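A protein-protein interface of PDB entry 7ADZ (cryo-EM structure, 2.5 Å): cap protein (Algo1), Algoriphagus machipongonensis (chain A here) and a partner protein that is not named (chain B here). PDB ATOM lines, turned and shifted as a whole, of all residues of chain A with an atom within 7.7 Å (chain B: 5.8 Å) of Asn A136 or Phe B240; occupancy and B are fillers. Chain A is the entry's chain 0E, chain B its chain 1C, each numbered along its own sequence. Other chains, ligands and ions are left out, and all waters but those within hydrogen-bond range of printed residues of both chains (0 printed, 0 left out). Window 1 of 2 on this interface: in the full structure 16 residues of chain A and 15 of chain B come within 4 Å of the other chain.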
ATOM      1  N   MET A   1       7.164 -14.127  30.432  1.00  0.00           N
ATOM      2  CA  MET A   1       7.706 -15.458  30.197  1.00  0.00           C
ATOM      3  C   MET A   1       8.591 -15.952  31.335  1.00  0.00           C
ATOM      4  O   MET A   1       9.266 -16.960  31.186  1.00  0.00           O
ATOM      5  CB  MET A   1       8.506 -15.484  28.893  1.00  0.00           C
ATOM      6  CG  MET A   1       7.669 -15.362  27.640  1.00  0.00           C
ATOM      7  SD  MET A   1       6.524 -16.742  27.427  1.00  0.00           S
ATOM      8  CE  MET A   1       7.659 -18.068  27.029  1.00  0.00           C
ATOM      9  N   THR A 118      15.070 -26.475  24.322  1.00  0.00           N
ATOM     10  CA  THR A 118      14.238 -25.886  23.281  1.00  0.00           C
ATOM     11  C   THR A 118      12.815 -26.416  23.387  1.00  0.00           C
ATOM     12  O   THR A 118      12.492 -27.239  24.243  1.00  0.00           O
ATOM     13  CB  THR A 118      14.782 -26.170  21.870  1.00  0.00           C
ATOM     14  OG1 THR A 118      15.025 -27.568  21.711  1.00  0.00           O
ATOM     15  CG2 THR A 118      16.059 -25.402  21.613  1.00  0.00           C
ATOM     16  N   GLN A 119      11.958 -25.935  22.483  1.00  0.00           N
ATOM     17  CA  GLN A 119      10.560 -26.361  22.466  1.00  0.00           C
ATOM     18  C   GLN A 119      10.417 -27.787  21.941  1.00  0.00           C
ATOM     19  O   GLN A 119       9.394 -28.439  22.172  1.00  0.00           O
ATOM     20  CB  GLN A 119       9.721 -25.386  21.632  1.00  0.00           C
ATOM     21  CG  GLN A 119       9.924 -25.500  20.126  1.00  0.00           C
ATOM     22  CD  GLN A 119      11.117 -24.722  19.616  1.00  0.00           C
ATOM     23  OE1 GLN A 119      11.875 -24.146  20.387  1.00  0.00           O
ATOM     24  NE2 GLN A 119      11.327 -24.765  18.319  1.00  0.00           N
ATOM     25  N   SER A 120      11.425 -28.281  21.221  1.00  0.00           N
ATOM     26  CA  SER A 120      11.410 -29.661  20.748  1.00  0.00           C
ATOM     27  C   SER A 120      12.117 -30.598  21.723  1.00  0.00           C
ATOM     28  O   SER A 120      11.917 -31.815  21.675  1.00  0.00           O
ATOM     29  CB  SER A 120      12.057 -29.741  19.369  1.00  0.00           C
ATOM     30  OG  SER A 120      11.528 -28.750  18.510  1.00  0.00           O
ATOM     31  N   ASN A 133       0.419 -19.711  26.490  1.00  0.00           N
ATOM     32  CA  ASN A 133       1.036 -18.573  25.820  1.00  0.00           C
ATOM     33  C   ASN A 133       2.422 -18.863  25.249  1.00  0.00           C
ATOM     34  O   ASN A 133       2.979 -17.995  24.573  1.00  0.00           O
ATOM     35  CB  ASN A 133       1.135 -17.385  26.781  1.00  0.00           C
ATOM     36  CG  ASN A 133      -0.143 -16.579  26.854  1.00  0.00           C
ATOM     37  OD1 ASN A 133      -0.681 -16.350  27.935  1.00  0.00           O
ATOM     38  ND2 ASN A 133      -0.632 -16.135  25.704  1.00  0.00           N
ATOM     39  N   VAL A 134       2.996 -20.037  25.496  1.00  0.00           N
ATOM     40  CA  VAL A 134       4.380 -20.301  25.102  1.00  0.00           C
ATOM     41  C   VAL A 134       4.419 -20.833  23.670  1.00  0.00           C
ATOM     42  O   VAL A 134       3.609 -21.687  23.284  1.00  0.00           O
ATOM     43  CB  VAL A 134       5.054 -21.259  26.108  1.00  0.00           C
ATOM     44  CG1 VAL A 134       4.260 -22.543  26.305  1.00  0.00           C
ATOM     45  CG2 VAL A 134       6.481 -21.573  25.707  1.00  0.00           C
ATOM     46  N   LYS A 135       5.316 -20.275  22.847  1.00  0.00           N
ATOM     47  CA  LYS A 135       5.463 -20.769  21.480  1.00  0.00           C
ATOM     48  C   LYS A 135       6.843 -21.347  21.158  1.00  0.00           C
ATOM     49  O   LYS A 135       6.968 -22.551  20.926  1.00  0.00           O
ATOM     50  CB  LYS A 135       5.141 -19.638  20.502  1.00  0.00           C
ATOM     51  CG  LYS A 135       3.914 -18.814  20.883  1.00  0.00           C
ATOM     52  CD  LYS A 135       4.016 -17.387  20.391  1.00  0.00           C
ATOM     53  CE  LYS A 135       3.753 -17.292  18.902  1.00  0.00           C
ATOM     54  NZ  LYS A 135       3.963 -15.917  18.383  1.00  0.00           N
ATOM     55  N   ASN A 136       7.888 -20.523  21.208  1.00  0.00           N
ATOM     56  CA  ASN A 136       9.237 -20.893  20.781  1.00  0.00           C
ATOM     57  C   ASN A 136      10.247 -20.346  21.780  1.00  0.00           C
ATOM     58  O   ASN A 136      10.180 -19.167  22.139  1.00  0.00           O
ATOM     59  CB  ASN A 136       9.558 -20.331  19.391  1.00  0.00           C
ATOM     60  CG  ASN A 136       9.055 -21.201  18.253  1.00  0.00           C
ATOM     61  OD1 ASN A 136       8.386 -22.207  18.459  1.00  0.00           O
ATOM     62  ND2 ASN A 136       9.385 -20.806  17.033  1.00  0.00           N
ATOM     63  N   PHE A 137      11.190 -21.180  22.215  1.00  0.00           N
ATOM     64  CA  PHE A 137      12.191 -20.712  23.167  1.00  0.00           C
ATOM     65  C   PHE A 137      13.499 -21.471  22.996  1.00  0.00           C
ATOM     66  O   PHE A 137      13.541 -22.561  22.428  1.00  0.00           O
ATOM     67  CB  PHE A 137      11.692 -20.808  24.624  1.00  0.00           C
ATOM     68  CG  PHE A 137      11.256 -22.188  25.056  1.00  0.00           C
ATOM     69  CD1 PHE A 137      12.153 -23.066  25.649  1.00  0.00           C
ATOM     70  CD2 PHE A 137       9.941 -22.586  24.908  1.00  0.00           C
ATOM     71  CE1 PHE A 137      11.751 -24.320  26.058  1.00  0.00           C
ATOM     72  CE2 PHE A 137       9.534 -23.838  25.315  1.00  0.00           C
ATOM     73  CZ  PHE A 137      10.437 -24.706  25.889  1.00  0.00           C
ATOM     74  N   ARG A 138      14.570 -20.865  23.508  1.00  0.00           N
ATOM     75  CA  ARG A 138      15.891 -21.475  23.577  1.00  0.00           C
ATOM     76  C   ARG A 138      16.689 -20.802  24.684  1.00  0.00           C
ATOM     77  O   ARG A 138      16.890 -19.587  24.637  1.00  0.00           O
ATOM     78  CB  ARG A 138      16.628 -21.339  22.242  1.00  0.00           C
ATOM     79  CG  ARG A 138      18.035 -21.893  22.272  1.00  0.00           C
ATOM     80  CD  ARG A 138      18.848 -21.456  21.074  1.00  0.00           C
ATOM     81  NE  ARG A 138      20.047 -22.273  20.931  1.00  0.00           N
ATOM     82  CZ  ARG A 138      21.258 -21.916  21.348  1.00  0.00           C
ATOM     83  NH1 ARG A 138      21.445 -20.742  21.929  1.00  0.00           N
ATOM     84  NH2 ARG A 138      22.284 -22.735  21.180  1.00  0.00           N
ATOM     85  N   VAL A 174      13.131 -13.604  26.341  1.00  0.00           N
ATOM     86  CA  VAL A 174      12.725 -12.513  25.457  1.00  0.00           C
ATOM     87  C   VAL A 174      11.365 -11.990  25.904  1.00  0.00           C
ATOM     88  O   VAL A 174      10.397 -12.752  25.992  1.00  0.00           O
ATOM     89  CB  VAL A 174      12.676 -12.964  23.990  1.00  0.00           C
ATOM     90  CG1 VAL A 174      12.237 -11.815  23.095  1.00  0.00           C
ATOM     91  CG2 VAL A 174      14.019 -13.498  23.552  1.00  0.00           C
ATOM     92  N   TYR B  19      10.676 -27.100   5.804  1.00  0.00           N
ATOM     93  CA  TYR B  19      11.435 -27.348   7.021  1.00  0.00           C
ATOM     94  C   TYR B  19      11.209 -26.240   8.045  1.00  0.00           C
ATOM     95  O   TYR B  19      11.192 -26.475   9.258  1.00  0.00           O
ATOM     96  CB  TYR B  19      12.911 -27.547   6.716  1.00  0.00           C
ATOM     97  CG  TYR B  19      13.755 -27.817   7.906  1.00  0.00           C
ATOM     98  CD1 TYR B  19      13.728 -29.043   8.532  1.00  0.00           C
ATOM     99  CD2 TYR B  19      14.581 -26.845   8.356  1.00  0.00           C
ATOM    100  CE1 TYR B  19      14.532 -29.263   9.615  1.00  0.00           C
ATOM    101  CE2 TYR B  19      15.375 -27.060   9.418  1.00  0.00           C
ATOM    102  CZ  TYR B  19      15.357 -28.254  10.054  1.00  0.00           C
ATOM    103  OH  TYR B  19      16.166 -28.434  11.133  1.00  0.00           O
ATOM    104  N   PHE B  20      11.122 -24.999   7.583  1.00  0.00           N
ATOM    105  CA  PHE B  20      10.999 -23.908   8.511  1.00  0.00           C
ATOM    106  C   PHE B  20       9.541 -23.530   8.747  1.00  0.00           C
ATOM    107  O   PHE B  20       9.199 -23.043   9.824  1.00  0.00           O
ATOM    108  CB  PHE B  20      11.731 -22.715   7.946  1.00  0.00           C
ATOM    109  CG  PHE B  20      13.190 -22.938   7.765  1.00  0.00           C
ATOM    110  CD1 PHE B  20      13.667 -23.344   6.549  1.00  0.00           C
ATOM    111  CD2 PHE B  20      14.080 -22.740   8.772  1.00  0.00           C
ATOM    112  CE1 PHE B  20      14.996 -23.555   6.335  1.00  0.00           C
ATOM    113  CE2 PHE B  20      15.428 -22.947   8.568  1.00  0.00           C
ATOM    114  CZ  PHE B  20      15.879 -23.357   7.343  1.00  0.00           C
ATOM    115  N   ASN B  22       6.494 -25.668   8.270  1.00  0.00           N
ATOM    116  CA  ASN B  22       5.524 -26.658   8.761  1.00  0.00           C
ATOM    117  C   ASN B  22       5.629 -26.831  10.261  1.00  0.00           C
ATOM    118  O   ASN B  22       6.641 -26.482  10.871  1.00  0.00           O
ATOM    119  CB  ASN B  22       5.673 -28.017   8.108  1.00  0.00           C
ATOM    120  CG  ASN B  22       5.269 -28.055   6.695  1.00  0.00           C
ATOM    121  OD1 ASN B  22       4.705 -27.101   6.144  1.00  0.00           O
ATOM    122  ND2 ASN B  22       5.491 -29.170   6.072  1.00  0.00           N
ATOM    123  N   ASP B  23       4.578 -27.354  10.881  1.00  0.00           N
ATOM    124  CA  ASP B  23       4.645 -27.631  12.311  1.00  0.00           C
ATOM    125  C   ASP B  23       4.328 -29.102  12.575  1.00  0.00           C
ATOM    126  O   ASP B  23       3.162 -29.498  12.708  1.00  0.00           O
ATOM    127  CB  ASP B  23       3.681 -26.739  13.095  1.00  0.00           C
ATOM    128  CG  ASP B  23       3.823 -26.933  14.602  1.00  0.00           C
ATOM    129  OD1 ASP B  23       4.549 -27.820  14.981  1.00  0.00           O
ATOM    130  OD2 ASP B  23       3.220 -26.207  15.358  1.00  0.00           O
ATOM    131  N   SER B  42       8.437 -16.138  11.890  1.00  0.00           N
ATOM    132  CA  SER B  42       9.711 -16.734  12.299  1.00  0.00           C
ATOM    133  C   SER B  42      10.585 -17.160  11.112  1.00  0.00           C
ATOM    134  O   SER B  42      11.614 -17.814  11.293  1.00  0.00           O
ATOM    135  CB  SER B  42       9.476 -17.938  13.191  1.00  0.00           C
ATOM    136  OG  SER B  42       8.882 -17.583  14.414  1.00  0.00           O
ATOM    137  N   THR B 238      11.271 -31.151  11.038  1.00  0.00           N
ATOM    138  CA  THR B 238      10.900 -29.748  11.024  1.00  0.00           C
ATOM    139  C   THR B 238      11.817 -29.014  11.962  1.00  0.00           C
ATOM    140  O   THR B 238      12.386 -29.634  12.861  1.00  0.00           O
ATOM    141  CB  THR B 238       9.433 -29.530  11.443  1.00  0.00           C
ATOM    142  OG1 THR B 238       9.263 -29.983  12.797  1.00  0.00           O
ATOM    143  CG2 THR B 238       8.470 -30.281  10.512  1.00  0.00           C
ATOM    144  N   LYS B 239      11.901 -27.703  11.831  1.00  0.00           N
ATOM    145  CA  LYS B 239      12.724 -26.936  12.756  1.00  0.00           C
ATOM    146  C   LYS B 239      12.058 -26.621  14.099  1.00  0.00           C
ATOM    147  O   LYS B 239      12.714 -26.676  15.135  1.00  0.00           O
ATOM    148  CB  LYS B 239      13.189 -25.635  12.134  1.00  0.00           C
ATOM    149  CG  LYS B 239      14.131 -24.875  13.028  1.00  0.00           C
ATOM    150  CD  LYS B 239      14.722 -23.700  12.336  1.00  0.00           C
ATOM    151  CE  LYS B 239      15.631 -22.903  13.266  1.00  0.00           C
ATOM    152  NZ  LYS B 239      16.869 -23.663  13.650  1.00  0.00           N
ATOM    153  N   PHE B 240      10.782 -26.233  14.085  1.00  0.00           N
ATOM    154  CA  PHE B 240      10.130 -25.784  15.316  1.00  0.00           C
ATOM    155  C   PHE B 240       9.012 -26.649  15.905  1.00  0.00           C
ATOM    156  O   PHE B 240       8.498 -26.316  16.968  1.00  0.00           O
ATOM    157  CB  PHE B 240       9.531 -24.404  15.092  1.00  0.00           C
ATOM    158  CG  PHE B 240      10.505 -23.353  14.726  1.00  0.00           C
ATOM    159  CD1 PHE B 240      10.539 -22.845  13.443  1.00  0.00           C
ATOM    160  CD2 PHE B 240      11.387 -22.863  15.650  1.00  0.00           C
ATOM    161  CE1 PHE B 240      11.424 -21.864  13.108  1.00  0.00           C
ATOM    162  CE2 PHE B 240      12.277 -21.884  15.316  1.00  0.00           C
ATOM    163  CZ  PHE B 240      12.292 -21.382  14.043  1.00  0.00           C
ATOM    164  N   GLY B 241       8.583 -27.703  15.230  1.00  0.00           N
ATOM    165  CA  GLY B 241       7.443 -28.471  15.731  1.00  0.00           C
ATOM    166  C   GLY B 241       7.805 -29.527  16.766  1.00  0.00           C
ATOM    167  O   GLY B 241       8.965 -29.685  17.146  1.00  0.00           O
ATOM    168  N   PHE B 242       6.794 -30.270  17.211  1.00  0.00           N
ATOM    169  CA  PHE B 242       6.976 -31.320  18.208  1.00  0.00           C
ATOM    170  C   PHE B 242       5.978 -32.451  18.082  1.00  0.00           C
ATOM    171  O   PHE B 242       4.767 -32.231  18.037  1.00  0.00           O
ATOM    172  CB  PHE B 242       6.888 -30.743  19.617  1.00  0.00           C
ATOM    173  CG  PHE B 242       6.965 -31.785  20.693  1.00  0.00           C
ATOM    174  CD1 PHE B 242       8.147 -32.399  21.017  1.00  0.00           C
ATOM    175  CD2 PHE B 242       5.825 -32.156  21.379  1.00  0.00           C
ATOM    176  CE1 PHE B 242       8.188 -33.362  21.989  1.00  0.00           C
ATOM    177  CE2 PHE B 242       5.870 -33.109  22.350  1.00  0.00           C
ATOM    178  CZ  PHE B 242       7.050 -33.716  22.653  1.00  0.00           C
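The side-chain amide nitrogen (NE2) of Gln A119 sits close to the backbone carbonyl oxygen (O) of Phe B240 (3.5 Å).
The backbone carbonyl oxygen (O) of Gly B241 lies within hydrogen-bond range of the side-chain hydroxyl (OG) of Ser A120.
OE1 of Gln A119 sits close to O of Phe A137.
The backbone NH of Lys B239 sits at hydrogen-bond distance from the backbone carbonyl oxygen of Tyr B19 (2.9 Å).
The side-chain hydroxyl (OG1) of Thr B238 sits at hydrogen-bond distance from the backbone NH (N) of Gly B241 (3.4 Å).
Among the printed residues, pairs that only touch across the chains: Asn A136 with Phe B240 (3.2 Å), Ser A120 with Phe B242 (3.9 Å) and Gln A119 with Lys B239 (3.96 Å).
Printed residues of chain B within 4 Å of Gln A119: Lys B239 (3.96 Å) and Phe B240 (3.3 Å).
Of the printed residues of chain B, Ser A120 touches Gly B241 and Phe B242.
Val A134 touches none of the printed residues of chain B.
Of the printed residues of chain B, Asn A136 touches Phe B240.
Val A174 touches none of the printed residues of chain B.
Of chain A, only Gln A119 (3.3 Å) and Asn A136 (3.2 Å) come within 4 Å of Phe B240.
Of chain A, only Ser A120 comes within 4 Å of Gly B241.
Of the printed residues of chain A, Phe B242 touches Ser A120.
The nearest printed residue of chain A that does not touch Phe B242 is Gln A119 (4.3 Å).
Of the 11 printed residues of chain A, 3 touch a printed residue of chain B.
Among the printed residues, 5 pairs touch across the chains.
Among the printed residues, no Asp or Glu carboxylate lies within 4 Å of a Lys or Arg side-chain nitrogen of the other chain.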
